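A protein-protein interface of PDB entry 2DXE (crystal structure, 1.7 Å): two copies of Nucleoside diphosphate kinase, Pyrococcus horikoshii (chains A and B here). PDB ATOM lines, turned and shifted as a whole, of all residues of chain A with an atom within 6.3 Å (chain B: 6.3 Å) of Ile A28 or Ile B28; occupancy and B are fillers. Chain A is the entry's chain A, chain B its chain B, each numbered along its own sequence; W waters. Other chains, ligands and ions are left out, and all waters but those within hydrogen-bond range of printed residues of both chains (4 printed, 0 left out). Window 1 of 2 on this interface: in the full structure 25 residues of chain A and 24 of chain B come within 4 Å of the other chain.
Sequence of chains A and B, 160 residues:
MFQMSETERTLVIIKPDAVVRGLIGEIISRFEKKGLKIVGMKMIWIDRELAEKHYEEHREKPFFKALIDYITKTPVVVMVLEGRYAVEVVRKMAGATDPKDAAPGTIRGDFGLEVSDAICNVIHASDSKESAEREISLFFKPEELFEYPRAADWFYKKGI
The backbone NH (N) of Leu B23 sits at hydrogen-bond distance from the side-chain carboxylate (OE2) of Glu A32 (3.4 Å).
The backbone NH (N) of Ile A24 is in hydrogen-bond range of the side-chain carboxylate (OE2) of Glu B32.
The backbone carbonyl oxygen (O) of Gly B25 sits close to the backbone carbonyl oxygen (O) of Gly A25, 3.5 Å away.
The backbone NH (N) of Gly A25 lies within hydrogen-bond range of the side-chain carboxylate (OE1) of Glu B32 (2.8 Å).
The backbone NH (N) of Gly B25 lies within hydrogen-bond range of the side-chain carboxylate (OE1) of Glu A32.
N of Ile B24 sits at hydrogen-bond distance from OE2 of Glu A32, at 2.9 Å.
The backbone NH (N) of Glu B26 is in hydrogen-bond range of the side-chain hydroxyl (OG) of Ser A29 (3.0 Å).
The backbone NH (N) of Glu A26 sits at hydrogen-bond distance from the side-chain hydroxyl (OG) of Ser B29.
OE2 of Glu B32 sits at hydrogen-bond distance from N of Leu A23.
N of Ile B14 is in hydrogen-bond range of O of Val B77 (2.8 Å).
O of Gly B25 is in hydrogen-bond range of OG of Ser B29, at 3.1 Å.
The side-chain hydroxyl (OG) of Ser A29 is in hydrogen-bond range of the backbone carbonyl oxygen (O) of Gly A25, at 3.2 Å.
N of Ile A14 lies within hydrogen-bond range of O of Val A77 (2.8 Å).
Among the printed residues, pairs that only touch across the chains: Ile A24 with Ile B38 (3.9 Å), Gly A25 with Ile B28 (3.7 Å), Gly A25 with Ser B29 (3.1 Å), Ile A28 with Gly B25 (3.7 Å), Ile A28 with Ile B28 (3.8 Å), Ser A29 with Gly B25 (3.1 Å), Ile A38 with Ile B24 (3.9 Å), Met A41 with Val B77 (3.8 Å) and Val A77 with Met B41 (3.8 Å).
Ile A28 touches two residues of chain B.
Of the printed residues of chain A, Ile B28 touches Gly A25 and Ile A28.
Of the printed residues of chain B, Ile A24 touches Glu B32 and Ile B38.
Of the printed residues of chain A, Met B41 touches Val A77 (3.8 Å).
Printed residues of chain A within 4 Å of Glu B32: Leu A23 (3.3 Å), Ile A24 (2.9 Å) and Gly A25 (2.8 Å).
Of the printed residues of chain B, Met A41 touches Val B77 (3.8 Å).
Of the printed residues of chain B, Ile A38 touches Ile B24 (3.9 Å).
The nearest residue of chain B that does not touch Ile A28 is Ile B24 (4.1 Å).
The nearest residue of chain A that does not touch Ile B28 is Ile A24 (4.2 Å).
Of the 16 printed residues of chain A, 10 touch a printed residue of chain B.
Printed residues of chain B that touch a printed residue of chain A: Leu B23, Ile B24, Gly B25, Glu B26, Ile B28, Ser B29, Glu B32, Ile B38, Met B41 and Val B77.
Hydrophobic or aromatic side chains of chain B within 4 Å of the printed part of chain A: Ile B24, Ile B28, Ile B38, Met B41 and Val B77.
Among the printed residues, 18 pairs touch across the chains.
Ile A24 touches Glu B32, and with the chains exchanged Glu A32 touches Ile B24.
Gly B25 touches its own counterpart, Gly A25.
Gly A25 touches Ser B29, and with the chains exchanged Ser A29 touches Gly B25.
Met A41 touches Val B77, and with the chains exchanged Val A77 touches Met B41.
Of the 18 pairs that touch across the chains among the printed residues, 18 have their exchanged pair printed and touching as well.
Water W1 lies within hydrogen-bond range of OE1 of Glu A32 (2.7 Å), OG of Ser A29 (2.7 Å), N of Glu B26 (3.0 Å) and N of Gly B25 (3.3 Å).
Water W4 lies within hydrogen-bond range of OG of Ser B29 (2.8 Å), OE1 of Glu B32 (2.8 Å), N of Glu A26 (3.0 Å) and N of Gly A25 (3.3 Å).
Water W3 lies within hydrogen-bond range of the side-chain hydroxyl (OG) of Ser B29 (2.8 Å), the side-chain hydroxyl (OG) of Ser A29 (2.8 Å), the backbone carbonyl oxygen (O) of Gly B25 (3.3 Å) and the backbone carbonyl oxygen (O) of Gly A25 (3.4 Å).
Water W2 lies within hydrogen-bond range of the side-chain carboxylate (OE2) of Glu A26 and the backbone carbonyl oxygen (O) of Ser B29.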
ATOM      1  N   ILE A  14     -10.287   5.028   3.490  1.00  0.00           N
ATOM      2  CA  ILE A  14     -11.155   5.029   4.656  1.00  0.00           C
ATOM      3  C   ILE A  14     -12.161   6.109   4.267  1.00  0.00           C
ATOM      4  O   ILE A  14     -11.850   7.300   4.252  1.00  0.00           O
ATOM      5  CB  ILE A  14     -10.380   5.400   5.933  1.00  0.00           C
ATOM      6  CG1 ILE A  14      -9.342   4.306   6.217  1.00  0.00           C
ATOM      7  CG2 ILE A  14     -11.338   5.555   7.107  1.00  0.00           C
ATOM      8  CD1 ILE A  14      -8.475   4.549   7.440  1.00  0.00           C
ATOM      9  N   LEU A  23     -13.625   6.225  13.136  1.00  0.00           N
ATOM     10  CA  LEU A  23     -13.158   4.845  13.057  1.00  0.00           C
ATOM     11  C   LEU A  23     -11.816   4.678  12.345  1.00  0.00           C
ATOM     12  O   LEU A  23     -11.398   3.556  12.076  1.00  0.00           O
ATOM     13  CB  LEU A  23     -14.204   3.991  12.335  1.00  0.00           C
ATOM     14  CG  LEU A  23     -15.607   3.941  12.940  1.00  0.00           C
ATOM     15  CD1 LEU A  23     -16.513   3.119  12.046  1.00  0.00           C
ATOM     16  CD2 LEU A  23     -15.547   3.354  14.336  1.00  0.00           C
ATOM     17  N   ILE A  24     -11.141   5.781  12.038  1.00  0.00           N
ATOM     18  CA  ILE A  24      -9.867   5.698  11.332  1.00  0.00           C
ATOM     19  C   ILE A  24      -8.863   4.791  12.035  1.00  0.00           C
ATOM     20  O   ILE A  24      -8.289   3.885  11.421  1.00  0.00           O
ATOM     21  CB  ILE A  24      -9.231   7.096  11.160  1.00  0.00           C
ATOM     22  CG1 ILE A  24     -10.134   7.973  10.287  1.00  0.00           C
ATOM     23  CG2 ILE A  24      -7.845   6.966  10.530  1.00  0.00           C
ATOM     24  CD1 ILE A  24      -9.674   9.421  10.172  1.00  0.00           C
ATOM     25  N   GLY A  25      -8.656   5.042  13.324  1.00  0.00           N
ATOM     26  CA  GLY A  25      -7.701   4.259  14.090  1.00  0.00           C
ATOM     27  C   GLY A  25      -8.008   2.778  14.166  1.00  0.00           C
ATOM     28  O   GLY A  25      -7.119   1.943  13.987  1.00  0.00           O
ATOM     29  N   GLU A  26      -9.266   2.445  14.436  1.00  0.00           N
ATOM     30  CA  GLU A  26      -9.668   1.048  14.544  1.00  0.00           C
ATOM     31  C   GLU A  26      -9.434   0.297  13.236  1.00  0.00           C
ATOM     32  O   GLU A  26      -9.004  -0.856  13.240  1.00  0.00           O
ATOM     33  CB  GLU A  26     -11.136   0.959  14.959  1.00  0.00           C
ATOM     34  CG  GLU A  26     -11.387   1.490  16.361  1.00  0.00           C
ATOM     35  CD  GLU A  26     -12.862   1.569  16.702  1.00  0.00           C
ATOM     36  OE1 GLU A  26     -13.535   0.519  16.687  1.00  0.00           O
ATOM     37  OE2 GLU A  26     -13.344   2.687  16.982  1.00  0.00           O
ATOM     38  N   ILE A  27      -9.702   0.958  12.116  1.00  0.00           N
ATOM     39  CA  ILE A  27      -9.495   0.332  10.823  1.00  0.00           C
ATOM     40  C   ILE A  27      -7.997   0.120  10.601  1.00  0.00           C
ATOM     41  O   ILE A  27      -7.566  -0.979  10.259  1.00  0.00           O
ATOM     42  CB  ILE A  27     -10.098   1.200   9.689  1.00  0.00           C
ATOM     43  CG1 ILE A  27     -11.620   1.243   9.844  1.00  0.00           C
ATOM     44  CG2 ILE A  27      -9.732   0.620   8.320  1.00  0.00           C
ATOM     45  CD1 ILE A  27     -12.315   2.244   8.922  1.00  0.00           C
ATOM     46  N   ILE A  28      -7.198   1.158  10.830  1.00  0.00           N
ATOM     47  CA  ILE A  28      -5.758   1.036  10.641  1.00  0.00           C
ATOM     48  C   ILE A  28      -5.185  -0.087  11.503  1.00  0.00           C
ATOM     49  O   ILE A  28      -4.390  -0.901  11.023  1.00  0.00           O
ATOM     50  CB  ILE A  28      -5.031   2.367  10.964  1.00  0.00           C
ATOM     51  CG1 ILE A  28      -5.374   3.406   9.885  1.00  0.00           C
ATOM     52  CG2 ILE A  28      -3.518   2.137  11.034  1.00  0.00           C
ATOM     53  CD1 ILE A  28      -4.829   4.797  10.143  1.00  0.00           C
ATOM     54  N   SER A  29      -5.601  -0.142  12.767  1.00  0.00           N
ATOM     55  CA  SER A  29      -5.109  -1.172  13.678  1.00  0.00           C
ATOM     56  C   SER A  29      -5.334  -2.592  13.173  1.00  0.00           C
ATOM     57  O   SER A  29      -4.496  -3.469  13.379  1.00  0.00           O
ATOM     58  CB  SER A  29      -5.756  -1.018  15.056  1.00  0.00           C
ATOM     59  OG  SER A  29      -5.219   0.095  15.739  1.00  0.00           O
ATOM     60  N   ARG A  30      -6.463  -2.835  12.518  1.00  0.00           N
ATOM     61  CA  ARG A  30      -6.727  -4.173  12.011  1.00  0.00           C
ATOM     62  C   ARG A  30      -5.668  -4.585  10.998  1.00  0.00           C
ATOM     63  O   ARG A  30      -5.235  -5.735  10.973  1.00  0.00           O
ATOM     64  CB  ARG A  30      -8.118  -4.242  11.386  1.00  0.00           C
ATOM     65  CG  ARG A  30      -9.203  -4.048  12.417  1.00  0.00           C
ATOM     66  CD  ARG A  30     -10.528  -4.578  11.950  1.00  0.00           C
ATOM     67  NE  ARG A  30     -11.528  -4.458  13.006  1.00  0.00           N
ATOM     68  CZ  ARG A  30     -12.678  -5.119  13.020  1.00  0.00           C
ATOM     69  NH1 ARG A  30     -12.973  -5.954  12.034  1.00  0.00           N
ATOM     70  NH2 ARG A  30     -13.528  -4.948  14.023  1.00  0.00           N
ATOM     71  N   PHE A  31      -5.242  -3.639  10.172  1.00  0.00           N
ATOM     72  CA  PHE A  31      -4.225  -3.934   9.176  1.00  0.00           C
ATOM     73  C   PHE A  31      -2.859  -4.125   9.830  1.00  0.00           C
ATOM     74  O   PHE A  31      -2.120  -5.046   9.486  1.00  0.00           O
ATOM     75  CB  PHE A  31      -4.184  -2.820   8.129  1.00  0.00           C
ATOM     76  CG  PHE A  31      -5.462  -2.690   7.343  1.00  0.00           C
ATOM     77  CD1 PHE A  31      -6.045  -3.811   6.756  1.00  0.00           C
ATOM     78  CD2 PHE A  31      -6.088  -1.456   7.200  1.00  0.00           C
ATOM     79  CE1 PHE A  31      -7.236  -3.710   6.037  1.00  0.00           C
ATOM     80  CE2 PHE A  31      -7.286  -1.342   6.479  1.00  0.00           C
ATOM     81  CZ  PHE A  31      -7.857  -2.470   5.900  1.00  0.00           C
ATOM     82  N   GLU A  32      -2.524  -3.265  10.786  1.00  0.00           N
ATOM     83  CA  GLU A  32      -1.242  -3.383  11.470  1.00  0.00           C
ATOM     84  C   GLU A  32      -1.136  -4.710  12.217  1.00  0.00           C
ATOM     85  O   GLU A  32      -0.090  -5.362  12.188  1.00  0.00           O
ATOM     86  CB  GLU A  32      -1.058  -2.229  12.462  1.00  0.00           C
ATOM     87  CG  GLU A  32      -0.826  -0.874  11.808  1.00  0.00           C
ATOM     88  CD  GLU A  32      -0.716   0.246  12.829  1.00  0.00           C
ATOM     89  OE1 GLU A  32      -1.716   0.508  13.530  1.00  0.00           O
ATOM     90  OE2 GLU A  32       0.366   0.859  12.933  1.00  0.00           O
ATOM     91  N   LYS A  33      -2.223  -5.106  12.879  1.00  0.00           N
ATOM     92  CA  LYS A  33      -2.255  -6.346  13.656  1.00  0.00           C
ATOM     93  C   LYS A  33      -2.132  -7.596  12.783  1.00  0.00           C
ATOM     94  O   LYS A  33      -1.636  -8.631  13.229  1.00  0.00           O
ATOM     95  CB  LYS A  33      -3.549  -6.404  14.479  1.00  0.00           C
ATOM     96  CG  LYS A  33      -3.646  -7.591  15.417  1.00  0.00           C
ATOM     97  CD  LYS A  33      -2.437  -7.679  16.343  1.00  0.00           C
ATOM     98  CE  LYS A  33      -2.284  -6.437  17.204  1.00  0.00           C
ATOM     99  NZ  LYS A  33      -3.439  -6.250  18.127  1.00  0.00           N
ATOM    100  N   ILE A  38       2.035  -0.148   6.400  1.00  0.00           N
ATOM    101  CA  ILE A  38       1.523   1.079   5.794  1.00  0.00           C
ATOM    102  C   ILE A  38       2.719   1.756   5.136  1.00  0.00           C
ATOM    103  O   ILE A  38       3.608   2.255   5.823  1.00  0.00           O
ATOM    104  CB  ILE A  38       0.930   2.031   6.851  1.00  0.00           C
ATOM    105  CG1 ILE A  38      -0.239   1.347   7.560  1.00  0.00           C
ATOM    106  CG2 ILE A  38       0.478   3.333   6.192  1.00  0.00           C
ATOM    107  CD1 ILE A  38      -0.758   2.112   8.760  1.00  0.00           C
ATOM    108  N   MET A  41       0.290   7.071   3.222  1.00  0.00           N
ATOM    109  CA  MET A  41      -0.975   7.461   3.839  1.00  0.00           C
ATOM    110  C   MET A  41      -1.140   8.963   3.998  1.00  0.00           C
ATOM    111  O   MET A  41      -0.198   9.677   4.342  1.00  0.00           O
ATOM    112  CB  MET A  41      -1.123   6.790   5.211  1.00  0.00           C
ATOM    113  CG  MET A  41      -2.385   7.194   5.966  1.00  0.00           C
ATOM    114  SD  MET A  41      -2.671   6.168   7.424  1.00  0.00           S
ATOM    115  CE  MET A  41      -1.325   6.689   8.464  1.00  0.00           C
ATOM    116  N   VAL A  77      -9.175   9.087   4.163  1.00  0.00           N
ATOM    117  CA  VAL A  77      -7.777   8.765   4.385  1.00  0.00           C
ATOM    118  C   VAL A  77      -7.416   7.711   3.358  1.00  0.00           C
ATOM    119  O   VAL A  77      -7.996   6.626   3.344  1.00  0.00           O
ATOM    120  CB  VAL A  77      -7.503   8.192   5.795  1.00  0.00           C
ATOM    121  CG1 VAL A  77      -6.042   7.764   5.896  1.00  0.00           C
ATOM    122  CG2 VAL A  77      -7.796   9.238   6.850  1.00  0.00           C
ATOM    123  N   MET A  79      -4.576   5.216   1.821  1.00  0.00           N
ATOM    124  CA  MET A  79      -3.363   4.583   2.307  1.00  0.00           C
ATOM    125  C   MET A  79      -2.986   3.385   1.461  1.00  0.00           C
ATOM    126  O   MET A  79      -3.838   2.752   0.838  1.00  0.00           O
ATOM    127  CB  MET A  79      -3.540   4.170   3.774  1.00  0.00           C
ATOM    128  CG  MET A  79      -4.597   3.112   4.023  1.00  0.00           C
ATOM    129  SD  MET A  79      -4.949   2.905   5.796  1.00  0.00           S
ATOM    130  CE  MET A  79      -3.403   2.402   6.401  1.00  0.00           C
ATOM    131  N   ILE B  14       3.541  10.709  15.286  1.00  0.00           N
ATOM    132  CA  ILE B  14       3.582   9.326  15.725  1.00  0.00           C
ATOM    133  C   ILE B  14       4.991   8.935  15.286  1.00  0.00           C
ATOM    134  O   ILE B  14       5.261   8.731  14.100  1.00  0.00           O
ATOM    135  CB  ILE B  14       2.512   8.471  15.023  1.00  0.00           C
ATOM    136  CG1 ILE B  14       1.124   8.967  15.440  1.00  0.00           C
ATOM    137  CG2 ILE B  14       2.693   6.999  15.392  1.00  0.00           C
ATOM    138  CD1 ILE B  14      -0.040   8.212  14.812  1.00  0.00           C
ATOM    139  N   LEU B  23       1.682   0.647  16.041  1.00  0.00           N
ATOM    140  CA  LEU B  23       0.770   1.283  16.984  1.00  0.00           C
ATOM    141  C   LEU B  23       0.044   2.511  16.440  1.00  0.00           C
ATOM    142  O   LEU B  23      -0.637   3.201  17.195  1.00  0.00           O
ATOM    143  CB  LEU B  23       1.535   1.690  18.244  1.00  0.00           C
ATOM    144  CG  LEU B  23       2.265   0.578  18.995  1.00  0.00           C
ATOM    145  CD1 LEU B  23       3.022   1.181  20.167  1.00  0.00           C
ATOM    146  CD2 LEU B  23       1.267  -0.468  19.466  1.00  0.00           C
ATOM    147  N   ILE B  24       0.181   2.787  15.147  1.00  0.00           N
ATOM    148  CA  ILE B  24      -0.467   3.960  14.561  1.00  0.00           C
ATOM    149  C   ILE B  24      -1.964   4.005  14.848  1.00  0.00           C
ATOM    150  O   ILE B  24      -2.480   5.009  15.342  1.00  0.00           O
ATOM    151  CB  ILE B  24      -0.271   4.007  13.030  1.00  0.00           C
ATOM    152  CG1 ILE B  24       1.210   4.205  12.698  1.00  0.00           C
ATOM    153  CG2 ILE B  24      -1.089   5.151  12.430  1.00  0.00           C
ATOM    154  CD1 ILE B  24       1.525   4.045  11.219  1.00  0.00           C
ATOM    155  N   GLY B  25      -2.655   2.916  14.532  1.00  0.00           N
ATOM    156  CA  GLY B  25      -4.092   2.864  14.743  1.00  0.00           C
ATOM    157  C   GLY B  25      -4.547   3.052  16.177  1.00  0.00           C
ATOM    158  O   GLY B  25      -5.499   3.789  16.442  1.00  0.00           O
ATOM    159  N   GLU B  26      -3.872   2.392  17.111  1.00  0.00           N
ATOM    160  CA  GLU B  26      -4.243   2.498  18.515  1.00  0.00           C
ATOM    161  C   GLU B  26      -4.091   3.914  19.040  1.00  0.00           C
ATOM    162  O   GLU B  26      -4.897   4.374  19.851  1.00  0.00           O
ATOM    163  CB  GLU B  26      -3.406   1.531  19.350  1.00  0.00           C
ATOM    164  CG  GLU B  26      -3.687   0.080  19.010  1.00  0.00           C
ATOM    165  CD  GLU B  26      -2.684  -0.866  19.628  1.00  0.00           C
ATOM    166  OE1 GLU B  26      -2.601  -0.911  20.871  1.00  0.00           O
ATOM    167  OE2 GLU B  26      -1.980  -1.562  18.866  1.00  0.00           O
ATOM    168  N   ILE B  27      -3.063   4.610  18.569  1.00  0.00           N
ATOM    169  CA  ILE B  27      -2.824   5.980  19.001  1.00  0.00           C
ATOM    170  C   ILE B  27      -3.908   6.893  18.434  1.00  0.00           C
ATOM    171  O   ILE B  27      -4.498   7.695  19.160  1.00  0.00           O
ATOM    172  CB  ILE B  27      -1.430   6.462  18.548  1.00  0.00           C
ATOM    173  CG1 ILE B  27      -0.355   5.699  19.327  1.00  0.00           C
ATOM    174  CG2 ILE B  27      -1.296   7.965  18.771  1.00  0.00           C
ATOM    175  CD1 ILE B  27       1.037   5.805  18.727  1.00  0.00           C
ATOM    176  N   ILE B  28      -4.184   6.758  17.142  1.00  0.00           N
ATOM    177  CA  ILE B  28      -5.211   7.578  16.512  1.00  0.00           C
ATOM    178  C   ILE B  28      -6.570   7.358  17.181  1.00  0.00           C
ATOM    179  O   ILE B  28      -7.305   8.312  17.431  1.00  0.00           O
ATOM    180  CB  ILE B  28      -5.317   7.268  14.999  1.00  0.00           C
ATOM    181  CG1 ILE B  28      -4.058   7.778  14.292  1.00  0.00           C
ATOM    182  CG2 ILE B  28      -6.586   7.893  14.416  1.00  0.00           C
ATOM    183  CD1 ILE B  28      -3.976   7.420  12.818  1.00  0.00           C
ATOM    184  N   SER B  29      -6.896   6.105  17.486  1.00  0.00           N
ATOM    185  CA  SER B  29      -8.177   5.811  18.122  1.00  0.00           C
ATOM    186  C   SER B  29      -8.345   6.526  19.456  1.00  0.00           C
ATOM    187  O   SER B  29      -9.450   6.934  19.809  1.00  0.00           O
ATOM    188  CB  SER B  29      -8.344   4.304  18.328  1.00  0.00           C
ATOM    189  OG  SER B  29      -8.563   3.648  17.093  1.00  0.00           O
ATOM    190  N   ARG B  30      -7.263   6.682  20.209  1.00  0.00           N
ATOM    191  CA  ARG B  30      -7.387   7.369  21.487  1.00  0.00           C
ATOM    192  C   ARG B  30      -7.842   8.807  21.297  1.00  0.00           C
ATOM    193  O   ARG B  30      -8.660   9.309  22.060  1.00  0.00           O
ATOM    194  CB  ARG B  30      -6.068   7.321  22.244  1.00  0.00           C
ATOM    195  CG  ARG B  30      -5.725   5.919  22.652  1.00  0.00           C
ATOM    196  CD  ARG B  30      -4.709   5.908  23.745  1.00  0.00           C
ATOM    197  NE  ARG B  30      -4.456   4.546  24.188  1.00  0.00           N
ATOM    198  CZ  ARG B  30      -3.881   4.247  25.344  1.00  0.00           C
ATOM    199  NH1 ARG B  30      -3.506   5.221  26.161  1.00  0.00           N
ATOM    200  NH2 ARG B  30      -3.684   2.979  25.674  1.00  0.00           N
ATOM    201  N   PHE B  31      -7.323   9.463  20.265  1.00  0.00           N
ATOM    202  CA  PHE B  31      -7.709  10.840  19.993  1.00  0.00           C
ATOM    203  C   PHE B  31      -9.141  10.902  19.464  1.00  0.00           C
ATOM    204  O   PHE B  31      -9.920  11.761  19.872  1.00  0.00           O
ATOM    205  CB  PHE B  31      -6.737  11.472  18.994  1.00  0.00           C
ATOM    206  CG  PHE B  31      -5.326  11.552  19.504  1.00  0.00           C
ATOM    207  CD1 PHE B  31      -5.057  12.102  20.754  1.00  0.00           C
ATOM    208  CD2 PHE B  31      -4.265  11.078  18.738  1.00  0.00           C
ATOM    209  CE1 PHE B  31      -3.752  12.180  21.237  1.00  0.00           C
ATOM    210  CE2 PHE B  31      -2.955  11.151  19.214  1.00  0.00           C
ATOM    211  CZ  PHE B  31      -2.701  11.701  20.461  1.00  0.00           C
ATOM    212  N   GLU B  32      -9.496   9.982  18.573  1.00  0.00           N
ATOM    213  CA  GLU B  32     -10.851   9.957  18.036  1.00  0.00           C
ATOM    214  C   GLU B  32     -11.871   9.715  19.152  1.00  0.00           C
ATOM    215  O   GLU B  32     -12.908  10.365  19.195  1.00  0.00           O
ATOM    216  CB  GLU B  32     -10.985   8.866  16.970  1.00  0.00           C
ATOM    217  CG  GLU B  32     -10.305   9.194  15.649  1.00  0.00           C
ATOM    218  CD  GLU B  32     -10.391   8.051  14.650  1.00  0.00           C
ATOM    219  OE1 GLU B  32      -9.841   6.966  14.940  1.00  0.00           O
ATOM    220  OE2 GLU B  32     -11.005   8.236  13.577  1.00  0.00           O
ATOM    221  N   LYS B  33     -11.561   8.787  20.054  1.00  0.00           N
ATOM    222  CA  LYS B  33     -12.457   8.451  21.164  1.00  0.00           C
ATOM    223  C   LYS B  33     -12.656   9.614  22.133  1.00  0.00           C
ATOM    224  O   LYS B  33     -13.723   9.756  22.730  1.00  0.00           O
ATOM    225  CB  LYS B  33     -11.908   7.248  21.933  1.00  0.00           C
ATOM    226  CG  LYS B  33     -12.943   6.192  22.267  1.00  0.00           C
ATOM    227  CD  LYS B  33     -13.372   5.460  21.001  1.00  0.00           C
ATOM    228  CE  LYS B  33     -14.234   4.249  21.305  1.00  0.00           C
ATOM    229  NZ  LYS B  33     -15.593   4.626  21.767  1.00  0.00           N
ATOM    230  N   ILE B  38      -9.386  14.979  13.583  1.00  0.00           N
ATOM    231  CA  ILE B  38      -8.162  14.937  12.788  1.00  0.00           C
ATOM    232  C   ILE B  38      -8.434  15.828  11.578  1.00  0.00           C
ATOM    233  O   ILE B  38      -9.243  15.482  10.718  1.00  0.00           O
ATOM    234  CB  ILE B  38      -7.866  13.510  12.293  1.00  0.00           C
ATOM    235  CG1 ILE B  38      -7.697  12.571  13.491  1.00  0.00           C
ATOM    236  CG2 ILE B  38      -6.625  13.515  11.405  1.00  0.00           C
ATOM    237  CD1 ILE B  38      -7.671  11.100  13.112  1.00  0.00           C
ATOM    238  N   MET B  41      -3.429  14.922   8.168  1.00  0.00           N
ATOM    239  CA  MET B  41      -2.618  13.753   8.495  1.00  0.00           C
ATOM    240  C   MET B  41      -1.926  13.143   7.286  1.00  0.00           C
ATOM    241  O   MET B  41      -2.481  13.096   6.188  1.00  0.00           O
ATOM    242  CB  MET B  41      -3.473  12.688   9.185  1.00  0.00           C
ATOM    243  CG  MET B  41      -2.726  11.397   9.463  1.00  0.00           C
ATOM    244  SD  MET B  41      -3.682  10.268  10.488  1.00  0.00           S
ATOM    245  CE  MET B  41      -5.153  10.097   9.498  1.00  0.00           C
ATOM    246  N   VAL B  77       4.060   9.484  11.243  1.00  0.00           N
ATOM    247  CA  VAL B  77       2.751   9.954  10.830  1.00  0.00           C
ATOM    248  C   VAL B  77       2.540  11.265  11.562  1.00  0.00           C
ATOM    249  O   VAL B  77       2.502  11.298  12.792  1.00  0.00           O
ATOM    250  CB  VAL B  77       1.618   8.970  11.213  1.00  0.00           C
ATOM    251  CG1 VAL B  77       0.266   9.597  10.902  1.00  0.00           C
ATOM    252  CG2 VAL B  77       1.776   7.673  10.439  1.00  0.00           C
ATOM    253  N   MET B  79       0.146  14.562  12.248  1.00  0.00           N
ATOM    254  CA  MET B  79      -1.272  14.873  12.172  1.00  0.00           C
ATOM    255  C   MET B  79      -1.617  16.077  13.021  1.00  0.00           C
ATOM    256  O   MET B  79      -0.921  16.406  13.986  1.00  0.00           O
ATOM    257  CB  MET B  79      -2.109  13.661  12.597  1.00  0.00           C
ATOM    258  CG  MET B  79      -1.909  13.215  14.028  1.00  0.00           C
ATOM    259  SD  MET B  79      -2.619  11.567  14.310  1.00  0.00           S
ATOM    260  CE  MET B  79      -4.315  11.883  14.092  1.00  0.00           C
HETATM  261  O   HOH W   1      -2.498  -0.046  16.050  1.00  0.00           O
HETATM  262  O   HOH W   2     -11.749   4.952  18.574  1.00  0.00           O
HETATM  263  O   HOH W   3      -7.357   1.136  17.247  1.00  0.00           O
HETATM  264  O   HOH W   4     -10.856   4.528  15.797  1.00  0.00           O
